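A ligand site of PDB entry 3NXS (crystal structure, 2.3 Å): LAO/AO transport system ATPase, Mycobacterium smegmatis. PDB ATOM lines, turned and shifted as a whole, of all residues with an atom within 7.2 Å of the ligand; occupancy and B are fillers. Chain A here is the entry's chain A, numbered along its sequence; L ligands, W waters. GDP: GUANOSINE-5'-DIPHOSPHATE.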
ATOM      1  N   GLY A  64     -27.192 -21.122   0.905  1.00  0.00           N
ATOM      2  CA  GLY A  64     -25.733 -21.040   1.069  1.00  0.00           C
ATOM      3  C   GLY A  64     -25.141 -22.174   0.228  1.00  0.00           C
ATOM      4  O   GLY A  64     -25.818 -23.173  -0.017  1.00  0.00           O
ATOM      5  N   VAL A  65     -23.897 -22.056  -0.194  1.00  0.00           N
ATOM      6  CA  VAL A  65     -23.242 -23.134  -0.976  1.00  0.00           C
ATOM      7  C   VAL A  65     -22.955 -24.368  -0.117  1.00  0.00           C
ATOM      8  O   VAL A  65     -22.891 -24.232   1.122  1.00  0.00           O
ATOM      9  CB  VAL A  65     -21.960 -22.622  -1.677  1.00  0.00           C
ATOM     10  CG1 VAL A  65     -22.336 -21.428  -2.655  1.00  0.00           C
ATOM     11  CG2 VAL A  65     -20.902 -22.215  -0.620  1.00  0.00           C
ATOM     12  N   PRO A  66     -22.822 -25.564  -0.748  1.00  0.00           N
ATOM     13  CA  PRO A  66     -22.486 -26.759   0.040  1.00  0.00           C
ATOM     14  C   PRO A  66     -21.257 -26.501   0.918  1.00  0.00           C
ATOM     15  O   PRO A  66     -20.349 -25.787   0.480  1.00  0.00           O
ATOM     16  CB  PRO A  66     -22.180 -27.823  -1.042  1.00  0.00           C
ATOM     17  CG  PRO A  66     -23.015 -27.416  -2.224  1.00  0.00           C
ATOM     18  CD  PRO A  66     -22.997 -25.881  -2.184  1.00  0.00           C
ATOM     19  N   GLY A  67     -21.269 -27.032   2.154  1.00  0.00           N
ATOM     20  CA  GLY A  67     -20.150 -26.831   3.084  1.00  0.00           C
ATOM     21  C   GLY A  67     -20.240 -25.607   3.978  1.00  0.00           C
ATOM     22  O   GLY A  67     -19.451 -25.451   4.945  1.00  0.00           O
ATOM     23  N   VAL A  68     -21.214 -24.739   3.701  1.00  0.00           N
ATOM     24  CA  VAL A  68     -21.415 -23.542   4.523  1.00  0.00           C
ATOM     25  C   VAL A  68     -21.880 -23.921   5.931  1.00  0.00           C
ATOM     26  O   VAL A  68     -21.557 -23.234   6.899  1.00  0.00           O
ATOM     27  CB  VAL A  68     -22.426 -22.564   3.853  1.00  0.00           C
ATOM     28  CG1 VAL A  68     -23.870 -22.955   4.174  1.00  0.00           C
ATOM     29  CG2 VAL A  68     -22.138 -21.119   4.238  1.00  0.00           C
ATOM     30  N   GLY A  69     -22.597 -25.039   6.070  1.00  0.00           N
ATOM     31  CA  GLY A  69     -23.229 -25.389   7.354  1.00  0.00           C
ATOM     32  C   GLY A  69     -24.725 -25.189   7.390  1.00  0.00           C
ATOM     33  O   GLY A  69     -25.294 -24.941   8.468  1.00  0.00           O
ATOM     34  N   LYS A  70     -25.388 -25.281   6.227  1.00  0.00           N
ATOM     35  CA  LYS A  70     -26.841 -25.061   6.115  1.00  0.00           C
ATOM     36  C   LYS A  70     -27.714 -26.128   6.874  1.00  0.00           C
ATOM     37  O   LYS A  70     -28.578 -25.773   7.637  1.00  0.00           O
ATOM     38  CB  LYS A  70     -27.229 -24.860   4.645  1.00  0.00           C
ATOM     39  CG  LYS A  70     -28.727 -24.613   4.394  1.00  0.00           C
ATOM     40  CD  LYS A  70     -28.978 -24.045   2.990  1.00  0.00           C
ATOM     41  CE  LYS A  70     -28.556 -24.975   1.852  1.00  0.00           C
ATOM     42  NZ  LYS A  70     -29.272 -26.282   1.945  1.00  0.00           N
ATOM     43  N   SER A  71     -27.452 -27.420   6.687  1.00  0.00           N
ATOM     44  CA  SER A  71     -28.158 -28.494   7.449  1.00  0.00           C
ATOM     45  C   SER A  71     -28.076 -28.314   8.950  1.00  0.00           C
ATOM     46  O   SER A  71     -29.086 -28.382   9.674  1.00  0.00           O
ATOM     47  CB  SER A  71     -27.573 -29.862   7.133  1.00  0.00           C
ATOM     48  OG  SER A  71     -27.581 -30.109   5.734  1.00  0.00           O
ATOM     49  N   THR A  72     -26.860 -28.106   9.425  1.00  0.00           N
ATOM     50  CA  THR A  72     -26.599 -27.859  10.829  1.00  0.00           C
ATOM     51  C   THR A  72     -27.343 -26.645  11.380  1.00  0.00           C
ATOM     52  O   THR A  72     -27.931 -26.691  12.492  1.00  0.00           O
ATOM     53  CB  THR A  72     -25.087 -27.712  11.055  1.00  0.00           C
ATOM     54  OG1 THR A  72     -24.420 -28.804  10.406  1.00  0.00           O
ATOM     55  CG2 THR A  72     -24.740 -27.709  12.542  1.00  0.00           C
ATOM     56  N   THR A  73     -27.346 -25.564  10.595  1.00  0.00           N
ATOM     57  CA  THR A  73     -28.019 -24.329  10.984  1.00  0.00           C
ATOM     58  C   THR A  73     -29.523 -24.520  11.051  1.00  0.00           C
ATOM     59  O   THR A  73     -30.159 -24.124  12.036  1.00  0.00           O
ATOM     60  CB  THR A  73     -27.722 -23.183   9.966  1.00  0.00           C
ATOM     61  OG1 THR A  73     -26.315 -22.852  10.040  1.00  0.00           O
ATOM     62  CG2 THR A  73     -28.564 -21.972  10.265  1.00  0.00           C
ATOM     63  N   ILE A  74     -30.082 -25.115   9.995  1.00  0.00           N
ATOM     64  CA  ILE A  74     -31.505 -25.363   9.921  1.00  0.00           C
ATOM     65  C   ILE A  74     -31.947 -26.278  11.060  1.00  0.00           C
ATOM     66  O   ILE A  74     -32.993 -26.072  11.664  1.00  0.00           O
ATOM     67  CB  ILE A  74     -31.893 -25.945   8.531  1.00  0.00           C
ATOM     68  CG1 ILE A  74     -31.907 -24.837   7.466  1.00  0.00           C
ATOM     69  CG2 ILE A  74     -33.234 -26.662   8.581  1.00  0.00           C
ATOM     70  CD1 ILE A  74     -31.890 -25.389   6.078  1.00  0.00           C
ATOM     71  N   ARG A 110     -30.257 -36.954   7.342  1.00  0.00           N
ATOM     72  CA  ARG A 110     -29.706 -35.622   7.142  1.00  0.00           C
ATOM     73  C   ARG A 110     -29.772 -34.696   8.367  1.00  0.00           C
ATOM     74  O   ARG A 110     -28.727 -34.246   8.861  1.00  0.00           O
ATOM     75  CB  ARG A 110     -30.324 -34.936   5.918  1.00  0.00           C
ATOM     76  CG  ARG A 110     -29.618 -33.634   5.579  1.00  0.00           C
ATOM     77  CD  ARG A 110     -30.055 -33.070   4.241  1.00  0.00           C
ATOM     78  NE  ARG A 110     -29.585 -31.692   4.096  1.00  0.00           N
ATOM     79  CZ  ARG A 110     -30.364 -30.612   4.084  1.00  0.00           C
ATOM     80  NH1 ARG A 110     -31.688 -30.727   4.172  1.00  0.00           N
ATOM     81  NH2 ARG A 110     -29.830 -29.404   3.972  1.00  0.00           N
ATOM     82  N   GLU A 156     -35.268 -24.127   1.890  1.00  0.00           N
ATOM     83  CA  GLU A 156     -33.842 -24.144   1.621  1.00  0.00           C
ATOM     84  C   GLU A 156     -33.494 -24.516   0.179  1.00  0.00           C
ATOM     85  O   GLU A 156     -34.203 -25.293  -0.454  1.00  0.00           O
ATOM     86  CB  GLU A 156     -33.119 -25.093   2.567  1.00  0.00           C
ATOM     87  CG  GLU A 156     -33.364 -26.529   2.241  1.00  0.00           C
ATOM     88  CD  GLU A 156     -32.488 -27.507   3.048  1.00  0.00           C
ATOM     89  OE1 GLU A 156     -32.986 -28.619   3.376  1.00  0.00           O
ATOM     90  OE2 GLU A 156     -31.319 -27.191   3.340  1.00  0.00           O
ATOM     91  N   LEU A 177     -26.258 -17.585   3.950  1.00  0.00           N
ATOM     92  CA  LEU A 177     -25.214 -18.102   4.798  1.00  0.00           C
ATOM     93  C   LEU A 177     -23.926 -18.091   4.025  1.00  0.00           C
ATOM     94  O   LEU A 177     -23.876 -18.569   2.882  1.00  0.00           O
ATOM     95  CB  LEU A 177     -25.515 -19.545   5.176  1.00  0.00           C
ATOM     96  CG  LEU A 177     -26.791 -19.858   6.003  1.00  0.00           C
ATOM     97  CD1 LEU A 177     -26.754 -21.329   6.409  1.00  0.00           C
ATOM     98  CD2 LEU A 177     -26.972 -18.972   7.244  1.00  0.00           C
ATOM     99  N   LEU A 179     -19.290 -18.007   4.375  1.00  0.00           N
ATOM    100  CA  LEU A 179     -18.121 -18.363   5.143  1.00  0.00           C
ATOM    101  C   LEU A 179     -17.077 -17.300   4.905  1.00  0.00           C
ATOM    102  O   LEU A 179     -16.988 -16.742   3.820  1.00  0.00           O
ATOM    103  CB  LEU A 179     -17.572 -19.710   4.668  1.00  0.00           C
ATOM    104  CG  LEU A 179     -18.329 -20.961   5.091  1.00  0.00           C
ATOM    105  CD1 LEU A 179     -17.462 -22.220   4.795  1.00  0.00           C
ATOM    106  CD2 LEU A 179     -18.703 -20.954   6.586  1.00  0.00           C
ATOM    107  N   ASN A 203     -21.063 -17.891   9.048  1.00  0.00           N
ATOM    108  CA  ASN A 203     -21.179 -19.052   9.922  1.00  0.00           C
ATOM    109  C   ASN A 203     -19.798 -19.573  10.263  1.00  0.00           C
ATOM    110  O   ASN A 203     -18.778 -19.022   9.820  1.00  0.00           O
ATOM    111  CB  ASN A 203     -22.050 -20.138   9.247  1.00  0.00           C
ATOM    112  CG  ASN A 203     -22.380 -21.312  10.175  1.00  0.00           C
ATOM    113  OD1 ASN A 203     -22.733 -21.116  11.342  1.00  0.00           O
ATOM    114  ND2 ASN A 203     -22.247 -22.531   9.664  1.00  0.00           N
ATOM    115  N   LYS A 204     -19.750 -20.628  11.063  1.00  0.00           N
ATOM    116  CA  LYS A 204     -18.489 -21.219  11.520  1.00  0.00           C
ATOM    117  C   LYS A 204     -17.590 -20.200  12.235  1.00  0.00           C
ATOM    118  O   LYS A 204     -16.376 -20.189  12.074  1.00  0.00           O
ATOM    119  CB  LYS A 204     -17.779 -21.896  10.345  1.00  0.00           C
ATOM    120  CG  LYS A 204     -18.585 -23.048   9.749  1.00  0.00           C
ATOM    121  CD  LYS A 204     -17.772 -23.890   8.779  1.00  0.00           C
ATOM    122  CE  LYS A 204     -18.690 -24.885   8.115  1.00  0.00           C
ATOM    123  NZ  LYS A 204     -17.918 -25.802   7.259  1.00  0.00           N
ATOM    124  N   ALA A 205     -18.223 -19.336  13.011  1.00  0.00           N
ATOM    125  CA  ALA A 205     -17.512 -18.338  13.806  1.00  0.00           C
ATOM    126  C   ALA A 205     -17.281 -18.916  15.191  1.00  0.00           C
ATOM    127  O   ALA A 205     -17.900 -18.495  16.175  1.00  0.00           O
ATOM    128  CB  ALA A 205     -18.322 -17.060  13.881  1.00  0.00           C
ATOM    129  N   ASP A 206     -16.395 -19.909  15.260  1.00  0.00           N
ATOM    130  CA  ASP A 206     -16.037 -20.626  16.490  1.00  0.00           C
ATOM    131  C   ASP A 206     -14.542 -20.965  16.428  1.00  0.00           C
ATOM    132  O   ASP A 206     -13.937 -20.899  15.332  1.00  0.00           O
ATOM    133  CB  ASP A 206     -16.876 -21.900  16.595  1.00  0.00           C
ATOM    134  CG  ASP A 206     -17.064 -22.575  15.254  1.00  0.00           C
ATOM    135  OD1 ASP A 206     -16.028 -22.951  14.635  1.00  0.00           O
ATOM    136  OD2 ASP A 206     -18.233 -22.658  14.798  1.00  0.00           O
ATOM    137  N   GLY A 207     -13.958 -21.315  17.584  1.00  0.00           N
ATOM    138  CA  GLY A 207     -12.552 -21.732  17.688  1.00  0.00           C
ATOM    139  C   GLY A 207     -11.582 -20.643  17.264  1.00  0.00           C
ATOM    140  O   GLY A 207     -11.858 -19.458  17.465  1.00  0.00           O
ATOM    141  N   HIS A 209     -11.002 -19.625  14.407  1.00  0.00           N
ATOM    142  CA  HIS A 209     -11.537 -18.908  13.252  1.00  0.00           C
ATOM    143  C   HIS A 209     -12.514 -17.748  13.577  1.00  0.00           C
ATOM    144  O   HIS A 209     -12.767 -16.897  12.718  1.00  0.00           O
ATOM    145  CB  HIS A 209     -12.173 -19.872  12.238  1.00  0.00           C
ATOM    146  CG  HIS A 209     -12.495 -19.228  10.938  1.00  0.00           C
ATOM    147  ND1 HIS A 209     -11.522 -18.854  10.030  1.00  0.00           N
ATOM    148  CD2 HIS A 209     -13.677 -18.859  10.391  1.00  0.00           C
ATOM    149  CE1 HIS A 209     -12.090 -18.286   8.993  1.00  0.00           C
ATOM    150  NE2 HIS A 209     -13.392 -18.285   9.176  1.00  0.00           N
ATOM    151  N   MET A 241     -22.279 -16.467  13.544  1.00  0.00           N
ATOM    152  CA  MET A 241     -22.979 -17.553  14.153  1.00  0.00           C
ATOM    153  C   MET A 241     -22.064 -18.730  14.206  1.00  0.00           C
ATOM    154  O   MET A 241     -21.167 -18.864  13.375  1.00  0.00           O
ATOM    155  CB  MET A 241     -24.178 -17.923  13.278  1.00  0.00           C
ATOM    156  CG  MET A 241     -25.265 -18.689  13.973  1.00  0.00           C
ATOM    157  SD  MET A 241     -26.623 -19.010  12.848  1.00  0.00           S
ATOM    158  CE  MET A 241     -25.803 -19.860  11.491  1.00  0.00           C
ATOM    159  N   SER A 242     -22.271 -19.567  15.217  1.00  0.00           N
ATOM    160  CA  SER A 242     -21.783 -20.926  15.162  1.00  0.00           C
ATOM    161  C   SER A 242     -23.010 -21.819  15.197  1.00  0.00           C
ATOM    162  O   SER A 242     -23.678 -21.941  16.235  1.00  0.00           O
ATOM    163  CB  SER A 242     -20.828 -21.249  16.328  1.00  0.00           C
ATOM    164  OG  SER A 242     -20.501 -22.628  16.340  1.00  0.00           O
ATOM    165  N   ALA A 243     -23.339 -22.416  14.063  1.00  0.00           N
ATOM    166  CA  ALA A 243     -24.389 -23.408  14.021  1.00  0.00           C
ATOM    167  C   ALA A 243     -24.088 -24.511  15.053  1.00  0.00           C
ATOM    168  O   ALA A 243     -24.981 -24.909  15.816  1.00  0.00           O
ATOM    169  CB  ALA A 243     -24.535 -23.976  12.623  1.00  0.00           C
ATOM    170  N   VAL A 244     -22.839 -24.982  15.100  1.00  0.00           N
ATOM    171  CA  VAL A 244     -22.480 -26.102  15.991  1.00  0.00           C
ATOM    172  C   VAL A 244     -22.626 -25.759  17.476  1.00  0.00           C
ATOM    173  O   VAL A 244     -23.283 -26.506  18.216  1.00  0.00           O
ATOM    174  CB  VAL A 244     -21.088 -26.710  15.665  1.00  0.00           C
ATOM    175  CG1 VAL A 244     -20.484 -27.399  16.889  1.00  0.00           C
ATOM    176  CG2 VAL A 244     -21.224 -27.728  14.545  1.00  0.00           C
ATOM    177  N   GLU A 245     -22.064 -24.632  17.904  1.00  0.00           N
ATOM    178  CA  GLU A 245     -22.155 -24.246  19.324  1.00  0.00           C
ATOM    179  C   GLU A 245     -23.482 -23.565  19.695  1.00  0.00           C
ATOM    180  O   GLU A 245     -23.806 -23.445  20.874  1.00  0.00           O
ATOM    181  CB  GLU A 245     -20.945 -23.407  19.720  1.00  0.00           C
ATOM    182  CG  GLU A 245     -19.647 -24.000  19.159  1.00  0.00           C
ATOM    183  CD  GLU A 245     -18.390 -23.409  19.742  1.00  0.00           C
ATOM    184  OE1 GLU A 245     -18.412 -22.271  20.295  1.00  0.00           O
ATOM    185  OE2 GLU A 245     -17.352 -24.102  19.624  1.00  0.00           O
ATOM    186  N   GLY A 246     -24.248 -23.120  18.698  1.00  0.00           N
ATOM    187  CA  GLY A 246     -25.523 -22.455  18.964  1.00  0.00           C
ATOM    188  C   GLY A 246     -25.456 -20.988  19.361  1.00  0.00           C
ATOM    189  O   GLY A 246     -26.476 -20.368  19.625  1.00  0.00           O
HETATM  190  PB  GDP L   1     -24.165 -27.933   4.389  1.00  0.00           P
HETATM  191  O1B GDP L   1     -25.472 -28.616   4.692  1.00  0.00           O
HETATM  192  O2B GDP L   1     -23.417 -28.615   3.270  1.00  0.00           O
HETATM  193  O3B GDP L   1     -24.327 -26.451   3.997  1.00  0.00           O
HETATM  194  O3A GDP L   1     -23.289 -27.993   5.699  1.00  0.00           O
HETATM  195  PA  GDP L   1     -23.511 -29.066   6.845  1.00  0.00           P
HETATM  196  O1A GDP L   1     -23.801 -30.449   6.303  1.00  0.00           O
HETATM  197  O2A GDP L   1     -24.519 -28.579   7.846  1.00  0.00           O
HETATM  198  O5' GDP L   1     -22.080 -29.010   7.556  1.00  0.00           O
HETATM  199  C5' GDP L   1     -20.895 -29.207   6.776  1.00  0.00           C
HETATM  200  C4' GDP L   1     -19.691 -29.360   7.699  1.00  0.00           C
HETATM  201  O4' GDP L   1     -19.447 -28.133   8.376  1.00  0.00           O
HETATM  202  C3' GDP L   1     -19.950 -30.438   8.762  1.00  0.00           C
HETATM  203  O3' GDP L   1     -18.736 -31.178   8.984  1.00  0.00           O
HETATM  204  C2' GDP L   1     -20.310 -29.664  10.003  1.00  0.00           C
HETATM  205  O2' GDP L   1     -19.951 -30.318  11.226  1.00  0.00           O
HETATM  206  C1' GDP L   1     -19.511 -28.381   9.796  1.00  0.00           C
HETATM  207  N9  GDP L   1     -20.162 -27.259  10.518  1.00  0.00           N
HETATM  208  C8  GDP L   1     -21.467 -26.908  10.472  1.00  0.00           C
HETATM  209  N7  GDP L   1     -21.703 -25.828  11.260  1.00  0.00           N
HETATM  210  C5  GDP L   1     -20.527 -25.484  11.805  1.00  0.00           C
HETATM  211  C6  GDP L   1     -20.048 -24.434  12.728  1.00  0.00           C
HETATM  212  O6  GDP L   1     -20.863 -23.595  13.181  1.00  0.00           O
HETATM  213  N1  GDP L   1     -18.743 -24.431  13.062  1.00  0.00           N
HETATM  214  C2  GDP L   1     -17.845 -25.326  12.587  1.00  0.00           C
HETATM  215  N2  GDP L   1     -16.536 -25.229  12.971  1.00  0.00           N
HETATM  216  N3  GDP L   1     -18.220 -26.312  11.722  1.00  0.00           N
HETATM  217  C4  GDP L   1     -19.512 -26.425  11.315  1.00  0.00           C
HETATM  218  O   HOH W   1     -25.715 -25.563   1.644  1.00  0.00           O
HETATM  219  O   HOH W   2     -27.589 -28.192   3.066  1.00  0.00           O
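Merely in contact with the ligand: Val 65, Pro 66, Val 68 and Asn 203. Hydrophobic or aromatic side chains that line the ligand: Val 68, Ala 243 and Val 244.
OD2 of Asp 206 is in hydrogen-bond range of OG of Ser 242. NZ of Lys 70 lies within salt-bridge range of OE2 of Glu 156 (2.6 Å). The backbone carbonyl oxygen of Gly 67 sits at hydrogen-bond distance from the side-chain amino group of Lys 204, at 2.8 Å. O of Val 68 sits at hydrogen-bond distance from ND2 of Asn 203, 2.9 Å away. The side-chain hydroxyl of Ser 71 sits at hydrogen-bond distance from the guanidinium group of Arg 110, at 2.9 Å. The backbone NH (N) of Ala 243 is in hydrogen-bond range of the side-chain amide oxygen (OD1) of Asn 203. O of Met 241 lies close to OD1 of Asn 203, at 3.4 Å. The backbone carbonyl oxygen of Gly 69 lies within hydrogen-bond range of the side-chain hydroxyl of Thr 73 (2.8 Å).
Water W2 lies within hydrogen-bond range of O1B of the ligand (2.7 Å), NH2 of Arg 110 (2.7 Å), NZ of Lys 70 (2.8 Å) and OG of Ser 71 (3.3 Å). Water W1 lies within hydrogen-bond range of an oxygen (O3B) of the ligand (2.9 Å), the backbone carbonyl oxygen of Gly 64 (2.9 Å) and the backbone carbonyl oxygen of Val 65 (3.2 Å).
N of Ala 243 is in hydrogen-bond range of O6 of the ligand (2.9 Å). The backbone NH (N) of Gly 69 sits at hydrogen-bond distance from an oxygen (O3B) of the ligand, 3.0 Å away. N of Thr 72 is in hydrogen-bond range of O2A of the ligand (2.9 Å). O3B of the ligand sits at hydrogen-bond distance from N of Lys 70, 2.7 Å away. OD2 of Asp 206 sits at hydrogen-bond distance from N1 of the ligand (2.5 Å). The side-chain hydroxyl (OG) of Ser 242 lies within hydrogen-bond range of an oxygen (O6) of the ligand (3.3 Å). An oxygen (O6) of the ligand sits at hydrogen-bond distance from the backbone NH (N) of Val 244, 3.1 Å away. OG of Ser 71 is in hydrogen-bond range of O1B of the ligand, at 2.8 Å. O2A of the ligand is in hydrogen-bond range of OG1 of Thr 72 (2.6 Å). NZ of Lys 204 is in hydrogen-bond range of O4' of the ligand. An oxygen (O1B) of the ligand lies within hydrogen-bond range of the backbone NH (N) of Ser 71 (3.1 Å). N of Gly 67 sits at hydrogen-bond distance from O2B of the ligand (2.9 Å).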
